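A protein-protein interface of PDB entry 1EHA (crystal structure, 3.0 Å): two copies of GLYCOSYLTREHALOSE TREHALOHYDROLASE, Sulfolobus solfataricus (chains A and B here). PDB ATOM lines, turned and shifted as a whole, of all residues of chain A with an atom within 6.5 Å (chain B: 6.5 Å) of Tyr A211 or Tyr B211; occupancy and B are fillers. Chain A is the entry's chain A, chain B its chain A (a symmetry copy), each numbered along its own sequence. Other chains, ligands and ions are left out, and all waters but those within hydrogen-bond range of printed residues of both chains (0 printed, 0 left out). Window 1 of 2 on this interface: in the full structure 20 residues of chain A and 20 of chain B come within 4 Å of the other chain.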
ATOM      1  N   SER A 208      32.493 -12.331  10.466  1.00  0.00           N
ATOM      2  CA  SER A 208      31.578 -12.215  11.585  1.00  0.00           C
ATOM      3  C   SER A 208      32.242 -12.332  12.940  1.00  0.00           C
ATOM      4  O   SER A 208      33.227 -13.048  13.120  1.00  0.00           O
ATOM      5  CB  SER A 208      30.352 -13.112  11.519  1.00  0.00           C
ATOM      6  OG  SER A 208      30.293 -13.798  12.743  1.00  0.00           O
ATOM      7  N   GLN A 209      31.653 -11.601  13.884  1.00  0.00           N
ATOM      8  CA  GLN A 209      32.116 -11.567  15.238  1.00  0.00           C
ATOM      9  C   GLN A 209      31.173 -12.313  16.114  1.00  0.00           C
ATOM     10  O   GLN A 209      31.493 -12.657  17.253  1.00  0.00           O
ATOM     11  CB  GLN A 209      32.267 -10.161  15.703  1.00  0.00           C
ATOM     12  CG  GLN A 209      31.755  -9.197  14.639  1.00  0.00           C
ATOM     13  CD  GLN A 209      32.090  -7.784  15.034  1.00  0.00           C
ATOM     14  OE1 GLN A 209      33.275  -7.462  15.263  1.00  0.00           O
ATOM     15  NE2 GLN A 209      31.038  -6.982  15.268  1.00  0.00           N
ATOM     16  N   LYS A 210      30.001 -12.571  15.552  1.00  0.00           N
ATOM     17  CA  LYS A 210      29.006 -13.359  16.230  1.00  0.00           C
ATOM     18  C   LYS A 210      29.623 -14.706  16.558  1.00  0.00           C
ATOM     19  O   LYS A 210      29.619 -15.143  17.703  1.00  0.00           O
ATOM     20  CB  LYS A 210      27.768 -13.580  15.355  1.00  0.00           C
ATOM     21  CG  LYS A 210      27.600 -12.532  14.250  1.00  0.00           C
ATOM     22  CD  LYS A 210      26.612 -12.946  13.155  1.00  0.00           C
ATOM     23  CE  LYS A 210      25.158 -12.556  13.455  1.00  0.00           C
ATOM     24  NZ  LYS A 210      24.165 -13.599  13.113  1.00  0.00           N
ATOM     25  N   TYR A 211      30.211 -15.337  15.529  1.00  0.00           N
ATOM     26  CA  TYR A 211      30.811 -16.646  15.673  1.00  0.00           C
ATOM     27  C   TYR A 211      32.341 -16.756  15.722  1.00  0.00           C
ATOM     28  O   TYR A 211      33.095 -15.829  15.396  1.00  0.00           O
ATOM     29  CB  TYR A 211      30.268 -17.628  14.645  1.00  0.00           C
ATOM     30  CG  TYR A 211      28.977 -17.206  14.022  1.00  0.00           C
ATOM     31  CD1 TYR A 211      27.825 -17.065  14.790  1.00  0.00           C
ATOM     32  CD2 TYR A 211      28.898 -16.980  12.645  1.00  0.00           C
ATOM     33  CE1 TYR A 211      26.629 -16.689  14.183  1.00  0.00           C
ATOM     34  CE2 TYR A 211      27.709 -16.594  12.024  1.00  0.00           C
ATOM     35  CZ  TYR A 211      26.567 -16.462  12.809  1.00  0.00           C
ATOM     36  OH  TYR A 211      25.380 -16.115  12.253  1.00  0.00           O
ATOM     37  N   LYS A 212      32.751 -17.973  16.128  1.00  0.00           N
ATOM     38  CA  LYS A 212      34.124 -18.408  16.256  1.00  0.00           C
ATOM     39  C   LYS A 212      34.288 -19.916  15.996  1.00  0.00           C
ATOM     40  O   LYS A 212      33.948 -20.772  16.826  1.00  0.00           O
ATOM     41  CB  LYS A 212      34.791 -17.945  17.553  1.00  0.00           C
ATOM     42  CG  LYS A 212      34.388 -18.740  18.791  1.00  0.00           C
ATOM     43  CD  LYS A 212      33.884 -17.855  19.936  1.00  0.00           C
ATOM     44  CE  LYS A 212      33.875 -18.556  21.295  1.00  0.00           C
ATOM     45  NZ  LYS A 212      33.606 -20.007  21.204  1.00  0.00           N
ATOM     46  N   THR A 213      34.795 -20.211  14.796  1.00  0.00           N
ATOM     47  CA  THR A 213      35.074 -21.558  14.320  1.00  0.00           C
ATOM     48  C   THR A 213      36.130 -22.159  15.260  1.00  0.00           C
ATOM     49  O   THR A 213      36.077 -21.895  16.465  1.00  0.00           O
ATOM     50  CB  THR A 213      35.529 -21.469  12.819  1.00  0.00           C
ATOM     51  OG1 THR A 213      36.885 -21.008  12.664  1.00  0.00           O
ATOM     52  CG2 THR A 213      34.561 -20.611  12.004  1.00  0.00           C
ATOM     53  N   GLY A 216      40.236 -19.737  14.180  1.00  0.00           N
ATOM     54  CA  GLY A 216      39.771 -18.384  14.142  1.00  0.00           C
ATOM     55  C   GLY A 216      38.265 -18.296  13.957  1.00  0.00           C
ATOM     56  O   GLY A 216      37.480 -18.853  14.729  1.00  0.00           O
ATOM     57  N   LEU A 217      37.875 -17.588  12.901  1.00  0.00           N
ATOM     58  CA  LEU A 217      36.476 -17.337  12.631  1.00  0.00           C
ATOM     59  C   LEU A 217      36.120 -17.185  11.165  1.00  0.00           C
ATOM     60  O   LEU A 217      36.867 -16.633  10.357  1.00  0.00           O
ATOM     61  CB  LEU A 217      36.034 -16.063  13.366  1.00  0.00           C
ATOM     62  CG  LEU A 217      37.124 -15.488  14.295  1.00  0.00           C
ATOM     63  CD1 LEU A 217      38.317 -14.903  13.512  1.00  0.00           C
ATOM     64  CD2 LEU A 217      36.502 -14.428  15.215  1.00  0.00           C
ATOM     65  N   THR A 218      34.925 -17.654  10.860  1.00  0.00           N
ATOM     66  CA  THR A 218      34.368 -17.604   9.531  1.00  0.00           C
ATOM     67  C   THR A 218      34.195 -16.149   9.142  1.00  0.00           C
ATOM     68  O   THR A 218      34.509 -15.264   9.934  1.00  0.00           O
ATOM     69  CB  THR A 218      33.030 -18.417   9.524  1.00  0.00           C
ATOM     70  OG1 THR A 218      32.465 -18.677   8.230  1.00  0.00           O
ATOM     71  CG2 THR A 218      32.015 -17.780  10.452  1.00  0.00           C
ATOM     72  N   PHE A 219      33.749 -15.934   7.908  1.00  0.00           N
ATOM     73  CA  PHE A 219      33.473 -14.626   7.381  1.00  0.00           C
ATOM     74  C   PHE A 219      32.115 -14.198   7.862  1.00  0.00           C
ATOM     75  O   PHE A 219      31.400 -14.934   8.549  1.00  0.00           O
ATOM     76  CB  PHE A 219      33.294 -14.656   5.868  1.00  0.00           C
ATOM     77  CG  PHE A 219      34.506 -14.995   5.108  1.00  0.00           C
ATOM     78  CD1 PHE A 219      35.532 -14.067   4.926  1.00  0.00           C
ATOM     79  CD2 PHE A 219      34.606 -16.254   4.527  1.00  0.00           C
ATOM     80  CE1 PHE A 219      36.672 -14.401   4.195  1.00  0.00           C
ATOM     81  CE2 PHE A 219      35.741 -16.607   3.800  1.00  0.00           C
ATOM     82  CZ  PHE A 219      36.765 -15.674   3.636  1.00  0.00           C
ATOM     83  N   ASN A 220      31.714 -13.041   7.390  1.00  0.00           N
ATOM     84  CA  ASN A 220      30.435 -12.516   7.746  1.00  0.00           C
ATOM     85  C   ASN A 220      29.431 -12.631   6.624  1.00  0.00           C
ATOM     86  O   ASN A 220      29.460 -11.846   5.707  1.00  0.00           O
ATOM     87  CB  ASN A 220      30.578 -11.055   8.170  1.00  0.00           C
ATOM     88  CG  ASN A 220      29.267 -10.566   8.647  1.00  0.00           C
ATOM     89  OD1 ASN A 220      28.581 -11.288   9.400  1.00  0.00           O
ATOM     90  ND2 ASN A 220      28.831  -9.460   8.056  1.00  0.00           N
ATOM     91  N   PHE A 221      28.510 -13.572   6.721  1.00  0.00           N
ATOM     92  CA  PHE A 221      27.512 -13.771   5.670  1.00  0.00           C
ATOM     93  C   PHE A 221      26.147 -13.306   6.081  1.00  0.00           C
ATOM     94  O   PHE A 221      25.247 -13.157   5.241  1.00  0.00           O
ATOM     95  CB  PHE A 221      27.415 -15.266   5.319  1.00  0.00           C
ATOM     96  CG  PHE A 221      28.779 -15.849   5.063  1.00  0.00           C
ATOM     97  CD1 PHE A 221      29.678 -16.033   6.115  1.00  0.00           C
ATOM     98  CD2 PHE A 221      29.181 -16.169   3.765  1.00  0.00           C
ATOM     99  CE1 PHE A 221      30.960 -16.531   5.885  1.00  0.00           C
ATOM    100  CE2 PHE A 221      30.455 -16.669   3.515  1.00  0.00           C
ATOM    101  CZ  PHE A 221      31.341 -16.839   4.580  1.00  0.00           C
ATOM    102  N   ASP A 222      26.046 -13.105   7.402  1.00  0.00           N
ATOM    103  CA  ASP A 222      24.844 -12.747   8.151  1.00  0.00           C
ATOM    104  C   ASP A 222      24.617 -11.276   8.496  1.00  0.00           C
ATOM    105  O   ASP A 222      23.669 -10.663   8.036  1.00  0.00           O
ATOM    106  CB  ASP A 222      24.862 -13.535   9.462  1.00  0.00           C
ATOM    107  CG  ASP A 222      24.218 -14.850   9.261  1.00  0.00           C
ATOM    108  OD1 ASP A 222      23.659 -15.184   8.216  1.00  0.00           O
ATOM    109  OD2 ASP A 222      24.290 -15.579  10.327  1.00  0.00           O
ATOM    110  N   ASP A 223      25.454 -10.750   9.378  1.00  0.00           N
ATOM    111  CA  ASP A 223      25.352  -9.395   9.911  1.00  0.00           C
ATOM    112  C   ASP A 223      25.524  -8.242   8.974  1.00  0.00           C
ATOM    113  O   ASP A 223      25.226  -8.306   7.787  1.00  0.00           O
ATOM    114  CB  ASP A 223      26.249  -9.168  11.142  1.00  0.00           C
ATOM    115  CG  ASP A 223      25.465  -8.950  12.399  1.00  0.00           C
ATOM    116  OD1 ASP A 223      24.270  -9.229  12.509  1.00  0.00           O
ATOM    117  OD2 ASP A 223      26.201  -8.430  13.351  1.00  0.00           O
ATOM    118  N   ILE A 258      28.846 -20.359   8.443  1.00  0.00           N
ATOM    119  CA  ILE A 258      27.640 -20.028   9.146  1.00  0.00           C
ATOM    120  C   ILE A 258      26.846 -18.900   8.550  1.00  0.00           C
ATOM    121  O   ILE A 258      27.340 -17.757   8.378  1.00  0.00           O
ATOM    122  CB  ILE A 258      27.812 -19.929  10.617  1.00  0.00           C
ATOM    123  CG1 ILE A 258      29.086 -20.693  11.027  1.00  0.00           C
ATOM    124  CG2 ILE A 258      26.575 -20.538  11.219  1.00  0.00           C
ATOM    125  CD1 ILE A 258      28.969 -21.541  12.295  1.00  0.00           C
ATOM    126  N   ASP A 259      25.603 -19.296   8.250  1.00  0.00           N
ATOM    127  CA  ASP A 259      24.611 -18.515   7.582  1.00  0.00           C
ATOM    128  C   ASP A 259      23.252 -18.758   8.178  1.00  0.00           C
ATOM    129  O   ASP A 259      22.882 -19.909   8.446  1.00  0.00           O
ATOM    130  CB  ASP A 259      24.532 -19.002   6.143  1.00  0.00           C
ATOM    131  CG  ASP A 259      24.555 -17.878   5.209  1.00  0.00           C
ATOM    132  OD1 ASP A 259      25.106 -16.832   5.512  1.00  0.00           O
ATOM    133  OD2 ASP A 259      23.941 -18.155   4.059  1.00  0.00           O
ATOM    134  N   THR A 260      22.493 -17.673   8.359  1.00  0.00           N
ATOM    135  CA  THR A 260      21.162 -17.780   8.932  1.00  0.00           C
ATOM    136  C   THR A 260      20.166 -17.251   7.978  1.00  0.00           C
ATOM    137  O   THR A 260      18.966 -17.362   8.194  1.00  0.00           O
ATOM    138  CB  THR A 260      21.060 -16.958  10.196  1.00  0.00           C
ATOM    139  OG1 THR A 260      21.128 -15.607   9.829  1.00  0.00           O
ATOM    140  CG2 THR A 260      22.227 -17.284  11.096  1.00  0.00           C
ATOM    141  N   SER B 208      25.845 -22.481  24.819  1.00  0.00           N
ATOM    142  CA  SER B 208      26.911 -22.503  23.836  1.00  0.00           C
ATOM    143  C   SER B 208      27.896 -21.363  23.970  1.00  0.00           C
ATOM    144  O   SER B 208      27.551 -20.251  24.367  1.00  0.00           O
ATOM    145  CB  SER B 208      26.461 -22.645  22.390  1.00  0.00           C
ATOM    146  OG  SER B 208      27.084 -21.610  21.675  1.00  0.00           O
ATOM    147  N   GLN B 209      29.137 -21.690  23.612  1.00  0.00           N
ATOM    148  CA  GLN B 209      30.225 -20.761  23.658  1.00  0.00           C
ATOM    149  C   GLN B 209      30.608 -20.363  22.277  1.00  0.00           C
ATOM    150  O   GLN B 209      31.319 -19.379  22.068  1.00  0.00           O
ATOM    151  CB  GLN B 209      31.387 -21.353  24.377  1.00  0.00           C
ATOM    152  CG  GLN B 209      31.105 -22.810  24.724  1.00  0.00           C
ATOM    153  CD  GLN B 209      32.196 -23.338  25.616  1.00  0.00           C
ATOM    154  OE1 GLN B 209      32.459 -22.762  26.692  1.00  0.00           O
ATOM    155  NE2 GLN B 209      32.935 -24.334  25.099  1.00  0.00           N
ATOM    156  N   LYS B 210      30.108 -21.142  21.329  1.00  0.00           N
ATOM    157  CA  LYS B 210      30.309 -20.846  19.936  1.00  0.00           C
ATOM    158  C   LYS B 210      29.762 -19.456  19.671  1.00  0.00           C
ATOM    159  O   LYS B 210      30.456 -18.592  19.147  1.00  0.00           O
ATOM    160  CB  LYS B 210      29.578 -21.847  19.035  1.00  0.00           C
ATOM    161  CG  LYS B 210      29.278 -23.185  19.717  1.00  0.00           C
ATOM    162  CD  LYS B 210      28.234 -24.031  18.981  1.00  0.00           C
ATOM    163  CE  LYS B 210      28.832 -24.953  17.909  1.00  0.00           C
ATOM    164  NZ  LYS B 210      28.053 -25.010  16.652  1.00  0.00           N
ATOM    165  N   TYR B 211      28.509 -19.239  20.100  1.00  0.00           N
ATOM    166  CA  TYR B 211      27.834 -17.975  19.889  1.00  0.00           C
ATOM    167  C   TYR B 211      27.674 -17.015  21.075  1.00  0.00           C
ATOM    168  O   TYR B 211      27.861 -17.358  22.251  1.00  0.00           O
ATOM    169  CB  TYR B 211      26.485 -18.166  19.210  1.00  0.00           C
ATOM    170  CG  TYR B 211      26.329 -19.488  18.528  1.00  0.00           C
ATOM    171  CD1 TYR B 211      27.142 -19.838  17.455  1.00  0.00           C
ATOM    172  CD2 TYR B 211      25.333 -20.380  18.935  1.00  0.00           C
ATOM    173  CE1 TYR B 211      26.964 -21.067  16.822  1.00  0.00           C
ATOM    174  CE2 TYR B 211      25.149 -21.617  18.318  1.00  0.00           C
ATOM    175  CZ  TYR B 211      25.971 -21.948  17.245  1.00  0.00           C
ATOM    176  OH  TYR B 211      25.816 -23.127  16.592  1.00  0.00           O
ATOM    177  N   LYS B 212      27.283 -15.787  20.687  1.00  0.00           N
ATOM    178  CA  LYS B 212      27.019 -14.664  21.558  1.00  0.00           C
ATOM    179  C   LYS B 212      25.940 -13.723  20.993  1.00  0.00           C
ATOM    180  O   LYS B 212      26.168 -12.937  20.063  1.00  0.00           O
ATOM    181  CB  LYS B 212      28.284 -13.928  22.004  1.00  0.00           C
ATOM    182  CG  LYS B 212      28.888 -13.009  20.947  1.00  0.00           C
ATOM    183  CD  LYS B 212      30.372 -13.285  20.687  1.00  0.00           C
ATOM    184  CE  LYS B 212      31.092 -12.143  19.969  1.00  0.00           C
ATOM    185  NZ  LYS B 212      30.223 -11.399  19.033  1.00  0.00           N
ATOM    186  N   THR B 213      24.742 -13.857  21.570  1.00  0.00           N
ATOM    187  CA  THR B 213      23.567 -13.066  21.238  1.00  0.00           C
ATOM    188  C   THR B 213      23.903 -11.601  21.554  1.00  0.00           C
ATOM    189  O   THR B 213      25.047 -11.189  21.332  1.00  0.00           O
ATOM    190  CB  THR B 213      22.344 -13.631  22.047  1.00  0.00           C
ATOM    191  OG1 THR B 213      22.355 -13.244  23.434  1.00  0.00           O
ATOM    192  CG2 THR B 213      22.247 -15.150  21.900  1.00  0.00           C
ATOM    193  N   GLY B 216      24.014 -11.408  26.437  1.00  0.00           N
ATOM    194  CA  GLY B 216      24.789 -12.568  26.754  1.00  0.00           C
ATOM    195  C   GLY B 216      24.822 -13.570  25.611  1.00  0.00           C
ATOM    196  O   GLY B 216      25.212 -13.257  24.483  1.00  0.00           O
ATOM    197  N   LEU B 217      24.390 -14.787  25.926  1.00  0.00           N
ATOM    198  CA  LEU B 217      24.437 -15.878  24.976  1.00  0.00           C
ATOM    199  C   LEU B 217      23.351 -16.924  25.142  1.00  0.00           C
ATOM    200  O   LEU B 217      22.933 -17.272  26.246  1.00  0.00           O
ATOM    201  CB  LEU B 217      25.799 -16.581  25.070  1.00  0.00           C
ATOM    202  CG  LEU B 217      26.787 -15.866  26.016  1.00  0.00           C
ATOM    203  CD1 LEU B 217      26.368 -15.971  27.497  1.00  0.00           C
ATOM    204  CD2 LEU B 217      28.196 -16.438  25.806  1.00  0.00           C
ATOM    205  N   THR B 218      22.944 -17.449  24.001  1.00  0.00           N
ATOM    206  CA  THR B 218      21.932 -18.472  23.916  1.00  0.00           C
ATOM    207  C   THR B 218      22.450 -19.713  24.616  1.00  0.00           C
ATOM    208  O   THR B 218      23.571 -19.707  25.118  1.00  0.00           O
ATOM    209  CB  THR B 218      21.589 -18.703  22.407  1.00  0.00           C
ATOM    210  OG1 THR B 218      20.431 -19.511  22.146  1.00  0.00           O
ATOM    211  CG2 THR B 218      22.801 -19.216  21.657  1.00  0.00           C
ATOM    212  N   PHE B 219      21.599 -20.733  24.680  1.00  0.00           N
ATOM    213  CA  PHE B 219      21.930 -22.006  25.257  1.00  0.00           C
ATOM    214  C   PHE B 219      22.688 -22.807  24.235  1.00  0.00           C
ATOM    215  O   PHE B 219      22.901 -22.382  23.095  1.00  0.00           O
ATOM    216  CB  PHE B 219      20.688 -22.858  25.487  1.00  0.00           C
ATOM    217  CG  PHE B 219      19.763 -22.341  26.507  1.00  0.00           C
ATOM    218  CD1 PHE B 219      20.045 -22.457  27.869  1.00  0.00           C
ATOM    219  CD2 PHE B 219      18.567 -21.762  26.099  1.00  0.00           C
ATOM    220  CE1 PHE B 219      19.155 -21.970  28.824  1.00  0.00           C
ATOM    221  CE2 PHE B 219      17.669 -21.262  27.039  1.00  0.00           C
ATOM    222  CZ  PHE B 219      17.968 -21.374  28.398  1.00  0.00           C
ATOM    223  N   ASN B 220      22.991 -24.025  24.617  1.00  0.00           N
ATOM    224  CA  ASN B 220      23.694 -24.907  23.743  1.00  0.00           C
ATOM    225  C   ASN B 220      22.799 -25.971  23.153  1.00  0.00           C
ATOM    226  O   ASN B 220      22.486 -26.931  23.814  1.00  0.00           O
ATOM    227  CB  ASN B 220      24.853 -25.560  24.494  1.00  0.00           C
ATOM    228  CG  ASN B 220      25.639 -26.375  23.543  1.00  0.00           C
ATOM    229  OD1 ASN B 220      25.911 -25.910  22.416  1.00  0.00           O
ATOM    230  ND2 ASN B 220      25.818 -27.640  23.901  1.00  0.00           N
ATOM    231  N   PHE B 221      22.430 -25.829  21.892  1.00  0.00           N
ATOM    232  CA  PHE B 221      21.546 -26.798  21.245  1.00  0.00           C
ATOM    233  C   PHE B 221      22.269 -27.662  20.255  1.00  0.00           C
ATOM    234  O   PHE B 221      21.745 -28.694  19.810  1.00  0.00           O
ATOM    235  CB  PHE B 221      20.422 -26.060  20.496  1.00  0.00           C
ATOM    236  CG  PHE B 221      19.760 -25.041  21.384  1.00  0.00           C
ATOM    237  CD1 PHE B 221      20.438 -23.879  21.755  1.00  0.00           C
ATOM    238  CD2 PHE B 221      18.479 -25.267  21.889  1.00  0.00           C
ATOM    239  CE1 PHE B 221      19.854 -22.949  22.614  1.00  0.00           C
ATOM    240  CE2 PHE B 221      17.876 -24.350  22.745  1.00  0.00           C
ATOM    241  CZ  PHE B 221      18.575 -23.197  23.108  1.00  0.00           C
ATOM    242  N   ASP B 222      23.476 -27.176  19.931  1.00  0.00           N
ATOM    243  CA  ASP B 222      24.400 -27.706  18.932  1.00  0.00           C
ATOM    244  C   ASP B 222      25.534 -28.615  19.405  1.00  0.00           C
ATOM    245  O   ASP B 222      25.589 -29.781  19.059  1.00  0.00           O
ATOM    246  CB  ASP B 222      25.030 -26.516  18.205  1.00  0.00           C
ATOM    247  CG  ASP B 222      24.181 -26.127  17.059  1.00  0.00           C
ATOM    248  OD1 ASP B 222      23.185 -26.758  16.702  1.00  0.00           O
ATOM    249  OD2 ASP B 222      24.638 -25.070  16.470  1.00  0.00           O
ATOM    250  N   ASP B 223      26.479 -28.035  20.131  1.00  0.00           N
ATOM    251  CA  ASP B 223      27.691 -28.701  20.597  1.00  0.00           C
ATOM    252  C   ASP B 223      27.557 -29.831  21.569  1.00  0.00           C
ATOM    253  O   ASP B 223      26.574 -30.561  21.601  1.00  0.00           O
ATOM    254  CB  ASP B 223      28.748 -27.717  21.129  1.00  0.00           C
ATOM    255  CG  ASP B 223      29.973 -27.661  20.269  1.00  0.00           C
ATOM    256  OD1 ASP B 223      30.013 -28.099  19.119  1.00  0.00           O
ATOM    257  OD2 ASP B 223      30.982 -27.099  20.892  1.00  0.00           O
ATOM    258  N   ILE B 258      19.983 -20.352  18.265  1.00  0.00           N
ATOM    259  CA  ILE B 258      20.855 -20.890  17.261  1.00  0.00           C
ATOM    260  C   ILE B 258      21.074 -22.375  17.339  1.00  0.00           C
ATOM    261  O   ILE B 258      21.534 -22.926  18.370  1.00  0.00           O
ATOM    262  CB  ILE B 258      22.102 -20.108  17.070  1.00  0.00           C
ATOM    263  CG1 ILE B 258      21.893 -18.684  17.621  1.00  0.00           C
ATOM    264  CG2 ILE B 258      22.365 -20.104  15.589  1.00  0.00           C
ATOM    265  CD1 ILE B 258      22.465 -17.553  16.763  1.00  0.00           C
ATOM    266  N   ASP B 259      20.716 -22.972  16.195  1.00  0.00           N
ATOM    267  CA  ASP B 259      20.699 -24.379  15.952  1.00  0.00           C
ATOM    268  C   ASP B 259      21.174 -24.684  14.559  1.00  0.00           C
ATOM    269  O   ASP B 259      20.777 -24.009  13.600  1.00  0.00           O
ATOM    270  CB  ASP B 259      19.251 -24.839  16.014  1.00  0.00           C
ATOM    271  CG  ASP B 259      19.116 -26.032  16.847  1.00  0.00           C
ATOM    272  OD1 ASP B 259      19.905 -26.247  17.754  1.00  0.00           O
ATOM    273  OD2 ASP B 259      18.072 -26.784  16.502  1.00  0.00           O
ATOM    274  N   THR B 260      22.003 -25.725  14.441  1.00  0.00           N
ATOM    275  CA  THR B 260      22.533 -26.115  13.145  1.00  0.00           C
ATOM    276  C   THR B 260      22.138 -27.507  12.845  1.00  0.00           C
ATOM    277  O   THR B 260      22.361 -28.003  11.748  1.00  0.00           O
ATOM    278  CB  THR B 260      24.043 -26.064  13.151  1.00  0.00           C
ATOM    279  OG1 THR B 260      24.498 -27.091  13.991  1.00  0.00           O
ATOM    280  CG2 THR B 260      24.493 -24.736  13.710  1.00  0.00           C
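Printed residues of chain A that touch a printed residue of chain B: Gln A209, Lys A210, Tyr A211 and Lys A212. Hydrophobic or aromatic side chains of chain A within 4 Å of the printed part of chain B: Tyr A211. Among the printed residues, 8 pairs touch across the chains.
Among the printed residues, merely in contact across the chains: Lys A212 with Lys B210, Lys A210 with Lys B212, Lys A210 with Lys B210, Tyr A211 with Tyr B211, Tyr A211 with Lys B210 and Lys A210 with Tyr B211.
Printed residues of chain B within 4 Å of Tyr A211: Lys B210 and Tyr B211. Printed residues of chain A within 4 Å of Tyr B211: Lys A210 and Tyr A211. Of the printed residues of chain A, Lys B210 touches Lys A210 (3.8 Å), Tyr A211 (3.998 Å) and Lys A212 (3.6 Å). Printed residues of chain B within 4 Å of Lys A212: Gln B209 and Lys B210. Printed residues of chain A within 4 Å of Gln B209: Lys A212. Of the printed residues of chain B, Lys A210 touches Lys B210, Tyr B211 and Lys B212. Of the printed residues of chain A, Lys B212 touches Gln A209 (2.5 Å) and Lys A210 (3.6 Å). Thr A213 touches none of the printed residues of chain B. Asp B223 touches none of the printed residues of chain A. The nearest printed residue of chain B that does not touch Tyr A211 is Ile B258 (5.0 Å). The nearest printed residue of chain A that does not touch Gln B209 is Lys A210 (6.3 Å).
Gln A209 touches Lys B212, and with the chains exchanged Lys A212 touches Gln B209. Lys A210 touches Tyr B211, and with the chains exchanged Tyr A211 touches Lys B210. Lys A210 touches Lys B212, and with the chains exchanged Lys A212 touches Lys B210. Tyr B211 touches its own counterpart, Tyr A211. 17 positions are printed for both chains. Of the 8 pairs that touch across the chains among the printed residues, 8 have their exchanged pair printed and touching as well.
The side-chain amino group (NZ) of Lys B212 lies within hydrogen-bond range of the backbone carbonyl oxygen (O) of Gln A209, 2.5 Å away. The side-chain amino group (NZ) of Lys A212 lies within hydrogen-bond range of the backbone carbonyl oxygen (O) of Gln B209, 2.5 Å away.
The side-chain hydroxyl (OG) of Ser A208 lies within hydrogen-bond range of the backbone NH (N) of Lys A210, at 3.1 Å. N of Tyr A211 is in hydrogen-bond range of OG of Ser A208. The side-chain amino group (NZ) of Lys A210 is in salt-bridge range of the side-chain carboxylate (OD2) of Asp A222, at 3.4 Å. OG of Ser B208 is in hydrogen-bond range of N of Lys B210 (3.1 Å). The backbone NH (N) of Tyr B211 lies within hydrogen-bond range of the side-chain hydroxyl (OG) of Ser B208, at 3.2 Å. The side-chain hydroxyl of Tyr B211 lies within hydrogen-bond range of the side-chain amino group of Lys B210 (2.9 Å).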
